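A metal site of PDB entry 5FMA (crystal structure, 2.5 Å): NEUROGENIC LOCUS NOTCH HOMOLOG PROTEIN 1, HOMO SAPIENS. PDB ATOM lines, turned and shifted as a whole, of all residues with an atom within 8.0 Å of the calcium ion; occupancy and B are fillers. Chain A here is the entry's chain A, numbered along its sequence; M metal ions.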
ATOM      1  N   GLY A 108      -5.576  18.364  29.718  1.00  0.00           N
ATOM      2  CA  GLY A 108      -6.378  19.343  29.000  1.00  0.00           C
ATOM      3  C   GLY A 108      -7.802  18.885  28.749  1.00  0.00           C
ATOM      4  O   GLY A 108      -8.709  19.717  28.703  1.00  0.00           O
ATOM      5  N   PHE A 109      -8.000  17.563  28.575  1.00  0.00           N
ATOM      6  CA  PHE A 109      -9.319  16.977  28.314  1.00  0.00           C
ATOM      7  C   PHE A 109      -9.913  16.306  29.558  1.00  0.00           C
ATOM      8  O   PHE A 109      -9.184  15.978  30.493  1.00  0.00           O
ATOM      9  CB  PHE A 109      -9.218  15.971  27.147  1.00  0.00           C
ATOM     10  CG  PHE A 109      -8.616  16.589  25.909  1.00  0.00           C
ATOM     11  CD1 PHE A 109      -9.400  17.260  24.990  1.00  0.00           C
ATOM     12  CD2 PHE A 109      -7.241  16.556  25.693  1.00  0.00           C
ATOM     13  CE1 PHE A 109      -8.830  17.881  23.873  1.00  0.00           C
ATOM     14  CE2 PHE A 109      -6.678  17.164  24.573  1.00  0.00           C
ATOM     15  CZ  PHE A 109      -7.473  17.813  23.672  1.00  0.00           C
ATOM     16  N   GLU A 116     -14.686  16.296  26.344  1.00  0.00           N
ATOM     17  CA  GLU A 116     -14.797  17.691  26.778  1.00  0.00           C
ATOM     18  C   GLU A 116     -13.425  18.341  26.981  1.00  0.00           C
ATOM     19  O   GLU A 116     -12.622  17.821  27.758  1.00  0.00           O
ATOM     20  CB  GLU A 116     -15.596  17.743  28.097  1.00  0.00           C
ATOM     21  CG  GLU A 116     -15.971  19.144  28.549  1.00  0.00           C
ATOM     22  CD  GLU A 116     -17.004  19.196  29.658  1.00  0.00           C
ATOM     23  OE1 GLU A 116     -16.947  18.332  30.563  1.00  0.00           O
ATOM     24  OE2 GLU A 116     -17.862  20.105  29.620  1.00  0.00           O
ATOM     25  N   ASN A 117     -13.185  19.495  26.324  1.00  0.00           N
ATOM     26  CA  ASN A 117     -11.946  20.259  26.470  1.00  0.00           C
ATOM     27  C   ASN A 117     -12.120  21.162  27.703  1.00  0.00           C
ATOM     28  O   ASN A 117     -13.132  21.871  27.783  1.00  0.00           O
ATOM     29  CB  ASN A 117     -11.695  21.115  25.213  1.00  0.00           C
ATOM     30  CG  ASN A 117     -10.334  21.787  25.146  1.00  0.00           C
ATOM     31  OD1 ASN A 117      -9.857  22.404  26.112  1.00  0.00           O
ATOM     32  ND2 ASN A 117      -9.700  21.763  23.985  1.00  0.00           N
ATOM     33  N   ILE A 118     -11.172  21.123  28.652  1.00  0.00           N
ATOM     34  CA  ILE A 118     -11.263  21.922  29.876  1.00  0.00           C
ATOM     35  C   ILE A 118     -11.150  23.410  29.523  1.00  0.00           C
ATOM     36  O   ILE A 118     -10.249  23.797  28.774  1.00  0.00           O
ATOM     37  CB  ILE A 118     -10.203  21.497  30.942  1.00  0.00           C
ATOM     38  CG1 ILE A 118     -10.406  20.029  31.385  1.00  0.00           C
ATOM     39  CG2 ILE A 118     -10.248  22.435  32.161  1.00  0.00           C
ATOM     40  CD1 ILE A 118      -9.159  19.393  32.048  1.00  0.00           C
ATOM     41  N   ASP A 119     -12.069  24.242  30.049  1.00  0.00           N
ATOM     42  CA  ASP A 119     -12.059  25.679  29.774  1.00  0.00           C
ATOM     43  C   ASP A 119     -10.968  26.346  30.612  1.00  0.00           C
ATOM     44  O   ASP A 119     -11.031  26.311  31.841  1.00  0.00           O
ATOM     45  CB  ASP A 119     -13.450  26.295  30.072  1.00  0.00           C
ATOM     46  CG  ASP A 119     -13.599  27.749  29.639  1.00  0.00           C
ATOM     47  OD1 ASP A 119     -12.943  28.158  28.669  1.00  0.00           O
ATOM     48  OD2 ASP A 119     -14.395  28.468  30.286  1.00  0.00           O
ATOM     49  N   ASP A 120      -9.976  26.945  29.943  1.00  0.00           N
ATOM     50  CA  ASP A 120      -8.829  27.613  30.577  1.00  0.00           C
ATOM     51  C   ASP A 120      -9.036  29.130  30.713  1.00  0.00           C
ATOM     52  O   ASP A 120      -8.132  29.822  31.162  1.00  0.00           O
ATOM     53  CB  ASP A 120      -7.553  27.308  29.778  1.00  0.00           C
ATOM     54  CG  ASP A 120      -7.244  25.838  29.676  1.00  0.00           C
ATOM     55  OD1 ASP A 120      -7.046  25.197  30.737  1.00  0.00           O
ATOM     56  OD2 ASP A 120      -7.201  25.307  28.551  1.00  0.00           O
ATOM     57  N   CYS A 121     -10.242  29.645  30.351  1.00  0.00           N
ATOM     58  CA  CYS A 121     -10.572  31.068  30.416  1.00  0.00           C
ATOM     59  C   CYS A 121     -11.036  31.626  31.780  1.00  0.00           C
ATOM     60  O   CYS A 121     -10.944  32.845  31.931  1.00  0.00           O
ATOM     61  CB  CYS A 121     -11.577  31.425  29.315  1.00  0.00           C
ATOM     62  SG  CYS A 121     -10.883  31.429  27.646  1.00  0.00           S
ATOM     63  N   VAL A 133     -10.047  33.118  23.979  1.00  0.00           N
ATOM     64  CA  VAL A 133     -10.259  31.996  23.074  1.00  0.00           C
ATOM     65  C   VAL A 133      -9.554  30.772  23.687  1.00  0.00           C
ATOM     66  O   VAL A 133      -8.339  30.799  23.840  1.00  0.00           O
ATOM     67  CB  VAL A 133      -9.722  32.297  21.644  1.00  0.00           C
ATOM     68  CG1 VAL A 133     -10.046  31.149  20.692  1.00  0.00           C
ATOM     69  CG2 VAL A 133     -10.278  33.622  21.127  1.00  0.00           C
ATOM     70  N   ASP A 134     -10.323  29.741  24.073  1.00  0.00           N
ATOM     71  CA  ASP A 134      -9.779  28.529  24.705  1.00  0.00           C
ATOM     72  C   ASP A 134      -8.953  27.686  23.734  1.00  0.00           C
ATOM     73  O   ASP A 134      -9.267  27.634  22.545  1.00  0.00           O
ATOM     74  CB  ASP A 134     -10.918  27.674  25.291  1.00  0.00           C
ATOM     75  CG  ASP A 134     -10.453  26.527  26.177  1.00  0.00           C
ATOM     76  OD1 ASP A 134      -9.796  26.806  27.208  1.00  0.00           O
ATOM     77  OD2 ASP A 134     -10.725  25.351  25.833  1.00  0.00           O
ATOM     78  N   GLY A 135      -7.921  27.043  24.259  1.00  0.00           N
ATOM     79  CA  GLY A 135      -7.034  26.144  23.527  1.00  0.00           C
ATOM     80  C   GLY A 135      -6.823  24.843  24.274  1.00  0.00           C
ATOM     81  O   GLY A 135      -7.639  24.469  25.123  1.00  0.00           O
ATOM     82  N   VAL A 136      -5.729  24.142  23.964  1.00  0.00           N
ATOM     83  CA  VAL A 136      -5.344  22.876  24.620  1.00  0.00           C
ATOM     84  C   VAL A 136      -4.233  23.242  25.624  1.00  0.00           C
ATOM     85  O   VAL A 136      -3.112  23.511  25.204  1.00  0.00           O
ATOM     86  CB  VAL A 136      -4.889  21.821  23.571  1.00  0.00           C
ATOM     87  CG1 VAL A 136      -4.268  20.586  24.255  1.00  0.00           C
ATOM     88  CG2 VAL A 136      -6.053  21.417  22.659  1.00  0.00           C
ATOM     89  N   ASN A 137      -4.578  23.314  26.934  1.00  0.00           N
ATOM     90  CA  ASN A 137      -3.679  23.700  28.040  1.00  0.00           C
ATOM     91  C   ASN A 137      -3.273  25.174  27.999  1.00  0.00           C
ATOM     92  O   ASN A 137      -2.337  25.568  28.693  1.00  0.00           O
ATOM     93  CB  ASN A 137      -2.437  22.756  28.165  1.00  0.00           C
ATOM     94  CG  ASN A 137      -2.703  21.502  28.920  1.00  0.00           C
ATOM     95  OD1 ASN A 137      -3.819  20.991  28.941  1.00  0.00           O
ATOM     96  ND2 ASN A 137      -1.672  20.971  29.583  1.00  0.00           N
ATOM     97  N   THR A 138      -4.019  26.017  27.265  1.00  0.00           N
ATOM     98  CA  THR A 138      -3.728  27.438  27.158  1.00  0.00           C
ATOM     99  C   THR A 138      -4.924  28.201  26.581  1.00  0.00           C
ATOM    100  O   THR A 138      -5.986  27.619  26.359  1.00  0.00           O
ATOM    101  CB  THR A 138      -2.417  27.684  26.347  1.00  0.00           C
ATOM    102  OG1 THR A 138      -2.145  29.090  26.294  1.00  0.00           O
ATOM    103  CG2 THR A 138      -2.465  27.082  24.926  1.00  0.00           C
ATOM    104  N   TYR A 139      -4.736  29.503  26.400  1.00  0.00           N
ATOM    105  CA  TYR A 139      -5.720  30.404  25.815  1.00  0.00           C
ATOM    106  C   TYR A 139      -4.980  31.535  25.125  1.00  0.00           C
ATOM    107  O   TYR A 139      -3.811  31.768  25.405  1.00  0.00           O
ATOM    108  CB  TYR A 139      -6.685  30.937  26.897  1.00  0.00           C
ATOM    109  CG  TYR A 139      -6.087  31.962  27.829  1.00  0.00           C
ATOM    110  CD1 TYR A 139      -5.375  31.577  28.955  1.00  0.00           C
ATOM    111  CD2 TYR A 139      -6.283  33.320  27.622  1.00  0.00           C
ATOM    112  CE1 TYR A 139      -4.819  32.515  29.822  1.00  0.00           C
ATOM    113  CE2 TYR A 139      -5.741  34.274  28.483  1.00  0.00           C
ATOM    114  CZ  TYR A 139      -5.016  33.869  29.593  1.00  0.00           C
ATOM    115  OH  TYR A 139      -4.505  34.807  30.450  1.00  0.00           O
HETATM  116 CA    CA M   1      -9.142  24.286  26.917  1.00  0.00          CA
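OD1 of Asn 117 binds the calcium ion (2.2 Å). The side-chain carboxylate (OD2) of Asp 134 binds the calcium ion (2.2 Å). O of Ile 118 is bound to the calcium ion. The calcium ion is bound by O of Gly 135, at 2.3 Å. OD1 of Asp 134 is bound to the calcium ion (2.6 Å). The side-chain carboxylate (OD2) of Asp 120 is bound to the calcium ion (2.7 Å). The calcium ion has six donor atoms within binding distance.
Five residues have an atom within 4 Å of the calcium ion: Asn 117, Ile 118, Asp 120, Asp 134 and Gly 135.
The backbone NH of Ile 118 sits at hydrogen-bond distance from the backbone carbonyl oxygen of Gly 108.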
